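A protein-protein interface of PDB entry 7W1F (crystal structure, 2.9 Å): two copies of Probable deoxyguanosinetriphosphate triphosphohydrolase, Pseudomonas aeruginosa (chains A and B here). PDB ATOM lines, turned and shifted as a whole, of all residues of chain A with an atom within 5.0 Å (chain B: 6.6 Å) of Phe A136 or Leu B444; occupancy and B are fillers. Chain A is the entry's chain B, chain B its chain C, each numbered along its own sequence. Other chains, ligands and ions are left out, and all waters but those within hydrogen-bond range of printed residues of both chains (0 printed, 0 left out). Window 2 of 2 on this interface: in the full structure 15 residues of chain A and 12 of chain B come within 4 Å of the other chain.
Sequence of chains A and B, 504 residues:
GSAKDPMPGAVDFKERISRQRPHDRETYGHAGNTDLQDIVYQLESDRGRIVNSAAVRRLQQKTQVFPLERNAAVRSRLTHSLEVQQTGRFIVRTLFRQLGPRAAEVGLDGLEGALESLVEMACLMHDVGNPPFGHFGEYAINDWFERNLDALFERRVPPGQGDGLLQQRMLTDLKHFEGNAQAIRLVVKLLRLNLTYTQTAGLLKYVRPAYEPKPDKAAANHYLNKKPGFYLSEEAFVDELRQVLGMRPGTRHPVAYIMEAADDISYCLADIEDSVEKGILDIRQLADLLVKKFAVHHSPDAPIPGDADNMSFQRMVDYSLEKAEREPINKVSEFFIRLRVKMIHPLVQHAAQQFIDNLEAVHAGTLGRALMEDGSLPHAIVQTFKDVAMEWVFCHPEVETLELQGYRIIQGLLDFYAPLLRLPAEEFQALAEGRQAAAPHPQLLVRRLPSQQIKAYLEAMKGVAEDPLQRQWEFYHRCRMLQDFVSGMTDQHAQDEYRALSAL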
ATOM      1  N   PRO A 132      31.383  23.018  15.903  1.00  0.00           N
ATOM      2  CA  PRO A 132      30.191  23.699  16.416  1.00  0.00           C
ATOM      3  C   PRO A 132      29.937  23.340  17.872  1.00  0.00           C
ATOM      4  O   PRO A 132      30.496  22.392  18.417  1.00  0.00           O
ATOM      5  CB  PRO A 132      29.070  23.179  15.515  1.00  0.00           C
ATOM      6  CG  PRO A 132      29.606  21.893  14.966  1.00  0.00           C
ATOM      7  CD  PRO A 132      31.044  22.193  14.729  1.00  0.00           C
ATOM      8  N   PHE A 133      29.047  24.119  18.489  1.00  0.00           N
ATOM      9  CA  PHE A 133      28.519  23.865  19.833  1.00  0.00           C
ATOM     10  C   PHE A 133      29.585  24.053  20.906  1.00  0.00           C
ATOM     11  O   PHE A 133      29.739  23.228  21.805  1.00  0.00           O
ATOM     12  CB  PHE A 133      27.883  22.478  19.912  1.00  0.00           C
ATOM     13  CG  PHE A 133      27.006  22.175  18.739  1.00  0.00           C
ATOM     14  CD1 PHE A 133      25.868  22.929  18.505  1.00  0.00           C
ATOM     15  CD2 PHE A 133      27.332  21.171  17.849  1.00  0.00           C
ATOM     16  CE1 PHE A 133      25.058  22.668  17.418  1.00  0.00           C
ATOM     17  CE2 PHE A 133      26.525  20.901  16.756  1.00  0.00           C
ATOM     18  CZ  PHE A 133      25.387  21.650  16.540  1.00  0.00           C
ATOM     19  N   GLY A 134      30.277  25.188  20.833  1.00  0.00           N
ATOM     20  CA  GLY A 134      31.243  25.561  21.853  1.00  0.00           C
ATOM     21  C   GLY A 134      32.296  24.496  22.039  1.00  0.00           C
ATOM     22  O   GLY A 134      32.754  23.855  21.084  1.00  0.00           O
ATOM     23  N   HIS A 135      32.680  24.281  23.292  1.00  0.00           N
ATOM     24  CA  HIS A 135      33.643  23.226  23.545  1.00  0.00           C
ATOM     25  C   HIS A 135      33.000  21.849  23.605  1.00  0.00           C
ATOM     26  O   HIS A 135      33.721  20.847  23.583  1.00  0.00           O
ATOM     27  CB  HIS A 135      34.447  23.515  24.807  1.00  0.00           C
ATOM     28  CG  HIS A 135      35.349  24.695  24.667  1.00  0.00           C
ATOM     29  ND1 HIS A 135      34.924  25.986  24.879  1.00  0.00           N
ATOM     30  CD2 HIS A 135      36.625  24.789  24.226  1.00  0.00           C
ATOM     31  CE1 HIS A 135      35.920  26.821  24.644  1.00  0.00           C
ATOM     32  NE2 HIS A 135      36.962  26.121  24.238  1.00  0.00           N
ATOM     33  N   PHE A 136      31.677  21.765  23.708  1.00  0.00           N
ATOM     34  CA  PHE A 136      31.048  20.452  23.702  1.00  0.00           C
ATOM     35  C   PHE A 136      31.100  19.781  22.331  1.00  0.00           C
ATOM     36  O   PHE A 136      30.941  18.558  22.252  1.00  0.00           O
ATOM     37  CB  PHE A 136      29.620  20.549  24.210  1.00  0.00           C
ATOM     38  CG  PHE A 136      29.528  20.567  25.687  1.00  0.00           C
ATOM     39  CD1 PHE A 136      29.007  19.487  26.367  1.00  0.00           C
ATOM     40  CD2 PHE A 136      29.987  21.653  26.407  1.00  0.00           C
ATOM     41  CE1 PHE A 136      28.934  19.498  27.748  1.00  0.00           C
ATOM     42  CE2 PHE A 136      29.916  21.668  27.788  1.00  0.00           C
ATOM     43  CZ  PHE A 136      29.387  20.592  28.456  1.00  0.00           C
ATOM     44  N   GLY A 137      31.290  20.537  21.250  1.00  0.00           N
ATOM     45  CA  GLY A 137      31.635  19.898  19.990  1.00  0.00           C
ATOM     46  C   GLY A 137      32.952  19.152  20.086  1.00  0.00           C
ATOM     47  O   GLY A 137      33.094  18.042  19.566  1.00  0.00           O
ATOM     48  N   GLU A 138      33.927  19.759  20.768  1.00  0.00           N
ATOM     49  CA  GLU A 138      35.204  19.113  21.055  1.00  0.00           C
ATOM     50  C   GLU A 138      35.016  17.894  21.950  1.00  0.00           C
ATOM     51  O   GLU A 138      35.540  16.810  21.659  1.00  0.00           O
ATOM     52  CB  GLU A 138      36.131  20.128  21.721  1.00  0.00           C
ATOM     53  CG  GLU A 138      37.407  19.572  22.279  1.00  0.00           C
ATOM     54  CD  GLU A 138      38.254  20.646  22.935  1.00  0.00           C
ATOM     55  OE1 GLU A 138      38.192  21.806  22.460  1.00  0.00           O
ATOM     56  OE2 GLU A 138      38.987  20.324  23.904  1.00  0.00           O
ATOM     57  N   TYR A 139      34.275  18.060  23.055  1.00  0.00           N
ATOM     58  CA  TYR A 139      34.086  16.962  24.002  1.00  0.00           C
ATOM     59  C   TYR A 139      33.410  15.766  23.345  1.00  0.00           C
ATOM     60  O   TYR A 139      33.845  14.625  23.516  1.00  0.00           O
ATOM     61  CB  TYR A 139      33.262  17.436  25.203  1.00  0.00           C
ATOM     62  CG  TYR A 139      33.899  18.538  26.030  1.00  0.00           C
ATOM     63  CD1 TYR A 139      35.273  18.751  26.014  1.00  0.00           C
ATOM     64  CD2 TYR A 139      33.118  19.369  26.835  1.00  0.00           C
ATOM     65  CE1 TYR A 139      35.843  19.764  26.772  1.00  0.00           C
ATOM     66  CE2 TYR A 139      33.688  20.378  27.597  1.00  0.00           C
ATOM     67  CZ  TYR A 139      35.045  20.569  27.559  1.00  0.00           C
ATOM     68  OH  TYR A 139      35.604  21.568  28.309  1.00  0.00           O
ATOM     69  N   ALA A 140      32.384  16.017  22.542  1.00  0.00           N
ATOM     70  CA  ALA A 140      31.626  14.932  21.930  1.00  0.00           C
ATOM     71  C   ALA A 140      32.502  14.044  21.050  1.00  0.00           C
ATOM     72  O   ALA A 140      32.316  12.822  21.016  1.00  0.00           O
ATOM     73  CB  ALA A 140      30.464  15.520  21.119  1.00  0.00           C
ATOM     74  N   GLU A 400      23.425  25.974  28.144  1.00  0.00           N
ATOM     75  CA  GLU A 400      23.680  24.590  28.516  1.00  0.00           C
ATOM     76  C   GLU A 400      22.759  23.628  27.781  1.00  0.00           C
ATOM     77  O   GLU A 400      23.111  22.454  27.600  1.00  0.00           O
ATOM     78  CB  GLU A 400      23.541  24.459  30.026  1.00  0.00           C
ATOM     79  CG  GLU A 400      24.548  25.329  30.746  1.00  0.00           C
ATOM     80  CD  GLU A 400      24.734  24.947  32.179  1.00  0.00           C
ATOM     81  OE1 GLU A 400      25.874  25.060  32.682  1.00  0.00           O
ATOM     82  OE2 GLU A 400      23.724  24.565  32.807  1.00  0.00           O
ATOM     83  N   GLU A 403      24.622  23.226  24.520  1.00  0.00           N
ATOM     84  CA  GLU A 403      25.790  22.372  24.709  1.00  0.00           C
ATOM     85  C   GLU A 403      25.375  20.904  24.745  1.00  0.00           C
ATOM     86  O   GLU A 403      25.929  20.068  24.022  1.00  0.00           O
ATOM     87  CB  GLU A 403      26.535  22.778  25.987  1.00  0.00           C
ATOM     88  CG  GLU A 403      27.018  24.237  25.991  1.00  0.00           C
ATOM     89  CD  GLU A 403      27.905  24.599  27.187  1.00  0.00           C
ATOM     90  OE1 GLU A 403      28.999  25.177  26.976  1.00  0.00           O
ATOM     91  OE2 GLU A 403      27.507  24.320  28.341  1.00  0.00           O
ATOM     92  N   LEU A 404      24.354  20.585  25.540  1.00  0.00           N
ATOM     93  CA  LEU A 404      23.869  19.213  25.609  1.00  0.00           C
ATOM     94  C   LEU A 404      23.302  18.743  24.270  1.00  0.00           C
ATOM     95  O   LEU A 404      23.552  17.611  23.843  1.00  0.00           O
ATOM     96  CB  LEU A 404      22.826  19.107  26.718  1.00  0.00           C
ATOM     97  CG  LEU A 404      22.599  17.740  27.342  1.00  0.00           C
ATOM     98  CD1 LEU A 404      23.928  17.104  27.645  1.00  0.00           C
ATOM     99  CD2 LEU A 404      21.803  17.923  28.622  1.00  0.00           C
ATOM    100  N   TYR A 407      25.955  17.971  21.873  1.00  0.00           N
ATOM    101  CA  TYR A 407      26.603  16.722  22.247  1.00  0.00           C
ATOM    102  C   TYR A 407      25.931  15.537  21.568  1.00  0.00           C
ATOM    103  O   TYR A 407      26.615  14.634  21.074  1.00  0.00           O
ATOM    104  CB  TYR A 407      26.584  16.562  23.761  1.00  0.00           C
ATOM    105  CG  TYR A 407      27.472  15.463  24.302  1.00  0.00           C
ATOM    106  CD1 TYR A 407      26.957  14.215  24.629  1.00  0.00           C
ATOM    107  CD2 TYR A 407      28.831  15.685  24.509  1.00  0.00           C
ATOM    108  CE1 TYR A 407      27.767  13.226  25.143  1.00  0.00           C
ATOM    109  CE2 TYR A 407      29.644  14.699  25.014  1.00  0.00           C
ATOM    110  CZ  TYR A 407      29.107  13.476  25.332  1.00  0.00           C
ATOM    111  OH  TYR A 407      29.914  12.487  25.843  1.00  0.00           O
ATOM    112  N   TYR B 417      19.367   9.911  31.281  1.00  0.00           N
ATOM    113  CA  TYR B 417      19.964  10.252  32.564  1.00  0.00           C
ATOM    114  C   TYR B 417      20.727   9.095  33.211  1.00  0.00           C
ATOM    115  O   TYR B 417      21.209   9.239  34.343  1.00  0.00           O
ATOM    116  CB  TYR B 417      18.882  10.777  33.508  1.00  0.00           C
ATOM    117  CG  TYR B 417      18.469  12.171  33.124  1.00  0.00           C
ATOM    118  CD1 TYR B 417      19.095  13.276  33.686  1.00  0.00           C
ATOM    119  CD2 TYR B 417      17.485  12.389  32.165  1.00  0.00           C
ATOM    120  CE1 TYR B 417      18.741  14.549  33.324  1.00  0.00           C
ATOM    121  CE2 TYR B 417      17.128  13.658  31.799  1.00  0.00           C
ATOM    122  CZ  TYR B 417      17.760  14.733  32.379  1.00  0.00           C
ATOM    123  OH  TYR B 417      17.407  16.010  32.019  1.00  0.00           O
ATOM    124  N   LEU B 431      28.804  16.732  42.007  1.00  0.00           N
ATOM    125  CA  LEU B 431      27.865  17.370  41.096  1.00  0.00           C
ATOM    126  C   LEU B 431      26.607  17.826  41.826  1.00  0.00           C
ATOM    127  O   LEU B 431      26.175  18.973  41.679  1.00  0.00           O
ATOM    128  CB  LEU B 431      27.521  16.397  39.970  1.00  0.00           C
ATOM    129  CG  LEU B 431      28.653  16.118  38.980  1.00  0.00           C
ATOM    130  CD1 LEU B 431      28.239  15.071  37.942  1.00  0.00           C
ATOM    131  CD2 LEU B 431      29.101  17.408  38.305  1.00  0.00           C
ATOM    132  N   ALA B 439      33.784  15.758  34.951  1.00  0.00           N
ATOM    133  CA  ALA B 439      32.859  15.408  33.875  1.00  0.00           C
ATOM    134  C   ALA B 439      31.927  16.568  33.534  1.00  0.00           C
ATOM    135  O   ALA B 439      31.142  16.994  34.392  1.00  0.00           O
ATOM    136  CB  ALA B 439      32.058  14.181  34.286  1.00  0.00           C
ATOM    137  N   PRO B 440      31.979  17.113  32.307  1.00  0.00           N
ATOM    138  CA  PRO B 440      31.086  18.226  31.948  1.00  0.00           C
ATOM    139  C   PRO B 440      29.720  17.750  31.483  1.00  0.00           C
ATOM    140  O   PRO B 440      28.711  18.423  31.723  1.00  0.00           O
ATOM    141  CB  PRO B 440      31.841  18.944  30.817  1.00  0.00           C
ATOM    142  CG  PRO B 440      33.185  18.247  30.702  1.00  0.00           C
ATOM    143  CD  PRO B 440      32.970  16.867  31.249  1.00  0.00           C
ATOM    144  N   HIS B 441      29.685  16.601  30.787  1.00  0.00           N
ATOM    145  CA  HIS B 441      28.408  16.068  30.322  1.00  0.00           C
ATOM    146  C   HIS B 441      27.520  15.624  31.480  1.00  0.00           C
ATOM    147  O   HIS B 441      26.334  15.999  31.499  1.00  0.00           O
ATOM    148  CB  HIS B 441      28.645  14.936  29.323  1.00  0.00           C
ATOM    149  CG  HIS B 441      27.391  14.254  28.878  1.00  0.00           C
ATOM    150  ND1 HIS B 441      26.354  14.930  28.283  1.00  0.00           N
ATOM    151  CD2 HIS B 441      26.995  12.963  28.969  1.00  0.00           C
ATOM    152  CE1 HIS B 441      25.378  14.084  28.009  1.00  0.00           C
ATOM    153  NE2 HIS B 441      25.740  12.884  28.416  1.00  0.00           N
ATOM    154  N   PRO B 442      27.993  14.820  32.443  1.00  0.00           N
ATOM    155  CA  PRO B 442      27.154  14.556  33.620  1.00  0.00           C
ATOM    156  C   PRO B 442      26.823  15.818  34.385  1.00  0.00           C
ATOM    157  O   PRO B 442      25.733  15.914  34.963  1.00  0.00           O
ATOM    158  CB  PRO B 442      28.008  13.580  34.443  1.00  0.00           C
ATOM    159  CG  PRO B 442      28.846  12.895  33.433  1.00  0.00           C
ATOM    160  CD  PRO B 442      29.198  13.972  32.454  1.00  0.00           C
ATOM    161  N   GLN B 443      27.732  16.799  34.396  1.00  0.00           N
ATOM    162  CA  GLN B 443      27.451  18.057  35.077  1.00  0.00           C
ATOM    163  C   GLN B 443      26.234  18.740  34.473  1.00  0.00           C
ATOM    164  O   GLN B 443      25.325  19.165  35.195  1.00  0.00           O
ATOM    165  CB  GLN B 443      28.661  18.991  34.978  1.00  0.00           C
ATOM    166  CG  GLN B 443      28.622  20.195  35.916  1.00  0.00           C
ATOM    167  CD  GLN B 443      29.725  21.196  35.615  1.00  0.00           C
ATOM    168  OE1 GLN B 443      30.839  21.086  36.124  1.00  0.00           O
ATOM    169  NE2 GLN B 443      29.416  22.179  34.772  1.00  0.00           N
ATOM    170  N   LEU B 444      26.166  18.793  33.138  1.00  0.00           N
ATOM    171  CA  LEU B 444      24.996  19.376  32.486  1.00  0.00           C
ATOM    172  C   LEU B 444      23.735  18.601  32.832  1.00  0.00           C
ATOM    173  O   LEU B 444      22.672  19.198  33.044  1.00  0.00           O
ATOM    174  CB  LEU B 444      25.193  19.421  30.971  1.00  0.00           C
ATOM    175  CG  LEU B 444      26.170  20.439  30.389  1.00  0.00           C
ATOM    176  CD1 LEU B 444      25.967  20.537  28.897  1.00  0.00           C
ATOM    177  CD2 LEU B 444      25.990  21.792  31.037  1.00  0.00           C
ATOM    178  N   LEU B 445      23.833  17.270  32.880  1.00  0.00           N
ATOM    179  CA  LEU B 445      22.673  16.464  33.236  1.00  0.00           C
ATOM    180  C   LEU B 445      22.217  16.755  34.661  1.00  0.00           C
ATOM    181  O   LEU B 445      21.012  16.812  34.936  1.00  0.00           O
ATOM    182  CB  LEU B 445      22.986  14.978  33.054  1.00  0.00           C
ATOM    183  CG  LEU B 445      23.087  14.488  31.607  1.00  0.00           C
ATOM    184  CD1 LEU B 445      23.232  12.987  31.556  1.00  0.00           C
ATOM    185  CD2 LEU B 445      21.877  14.921  30.793  1.00  0.00           C
ATOM    186  N   VAL B 446      23.162  16.933  35.585  1.00  0.00           N
ATOM    187  CA  VAL B 446      22.772  17.216  36.961  1.00  0.00           C
ATOM    188  C   VAL B 446      22.131  18.598  37.066  1.00  0.00           C
ATOM    189  O   VAL B 446      21.123  18.772  37.759  1.00  0.00           O
ATOM    190  CB  VAL B 446      23.974  17.050  37.913  1.00  0.00           C
ATOM    191  CG1 VAL B 446      23.630  17.534  39.307  1.00  0.00           C
ATOM    192  CG2 VAL B 446      24.388  15.608  37.972  1.00  0.00           C
ATOM    193  N   ARG B 447      22.678  19.594  36.361  1.00  0.00           N
ATOM    194  CA  ARG B 447      22.131  20.952  36.435  1.00  0.00           C
ATOM    195  C   ARG B 447      20.704  21.059  35.889  1.00  0.00           C
ATOM    196  O   ARG B 447      20.026  22.053  36.165  1.00  0.00           O
ATOM    197  CB  ARG B 447      23.043  21.939  35.694  1.00  0.00           C
ATOM    198  CG  ARG B 447      24.330  22.291  36.437  1.00  0.00           C
ATOM    199  CD  ARG B 447      25.231  23.199  35.605  1.00  0.00           C
ATOM    200  N   ARG B 448      20.239  20.078  35.113  1.00  0.00           N
ATOM    201  CA  ARG B 448      18.853  20.039  34.648  1.00  0.00           C
ATOM    202  C   ARG B 448      17.886  19.484  35.691  1.00  0.00           C
ATOM    203  O   ARG B 448      16.676  19.707  35.584  1.00  0.00           O
ATOM    204  CB  ARG B 448      18.761  19.202  33.377  1.00  0.00           C
ATOM    205  CG  ARG B 448      19.561  19.750  32.217  1.00  0.00           C
ATOM    206  CD  ARG B 448      19.224  18.949  30.968  1.00  0.00           C
ATOM    207  NE  ARG B 448      17.936  19.276  30.375  1.00  0.00           N
ATOM    208  CZ  ARG B 448      17.769  20.188  29.436  1.00  0.00           C
ATOM    209  NH1 ARG B 448      18.813  20.862  28.983  1.00  0.00           N
ATOM    210  NH2 ARG B 448      16.567  20.407  28.943  1.00  0.00           N
ATOM    211  N   LEU B 449      18.380  18.734  36.666  1.00  0.00           N
ATOM    212  CA  LEU B 449      17.499  18.099  37.628  1.00  0.00           C
ATOM    213  C   LEU B 449      16.888  19.135  38.573  1.00  0.00           C
ATOM    214  O   LEU B 449      17.523  20.145  38.898  1.00  0.00           O
ATOM    215  CB  LEU B 449      18.263  17.047  38.422  1.00  0.00           C
ATOM    216  CG  LEU B 449      18.753  15.894  37.550  1.00  0.00           C
ATOM    217  CD1 LEU B 449      19.474  14.818  38.386  1.00  0.00           C
ATOM    218  CD2 LEU B 449      17.587  15.296  36.773  1.00  0.00           C
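No position is printed for both chains.
Of the 11 pairs that touch across the chains among the printed residues, none has its exchanged pair printed and touching as well.
Printed residues of chain B within 4 Å of Phe A136: Pro B440 and Leu B444.
Leu B444 touches four residues of chain A.
Printed residues of chain B within 4 Å of Glu A400: Leu B444 (3.6 Å) and Arg B447 (3.5 Å).
Of the printed residues of chain A, His B441 touches Leu A404 and Tyr A407.
Of the printed residues of chain A, Arg B448 touches Leu A404 (3.6 Å).
Printed residues of chain B within 4 Å of Glu A403: Leu B444 (3.7 Å).
Of the printed residues of chain B, Tyr A407 touches His B441.
Glu A138 touches none of the printed residues of chain B.
The nearest printed residue of chain A that does not touch Leu B444 is Tyr A407 (6.5 Å).
Among the printed residues, merely in contact across the chains: Phe A136 with Pro B440 (3.8 Å), Phe A136 with Leu B444 (3.3 Å), Tyr A139 with Pro B440 (3.8 Å), Glu A400 with Leu B444 (3.6 Å), Glu A400 with Arg B447 (3.5 Å), Glu A403 with Leu B444 (3.7 Å), Leu A404 with His B441 (3.3 Å), Leu A404 with Leu B444 (3.7 Å), Leu A404 with Leu B445 (3.7 Å), Leu A404 with Arg B448 (3.6 Å) and Tyr A407 with His B441 (3.7 Å).
Printed residues of chain A that touch a printed residue of chain B: Phe A136, Tyr A139, Glu A400, Glu A403, Leu A404 and Tyr A407.
Among the printed residues, no Asp or Glu carboxylate lies within 4 Å of a Lys or Arg side-chain nitrogen of the other chain.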
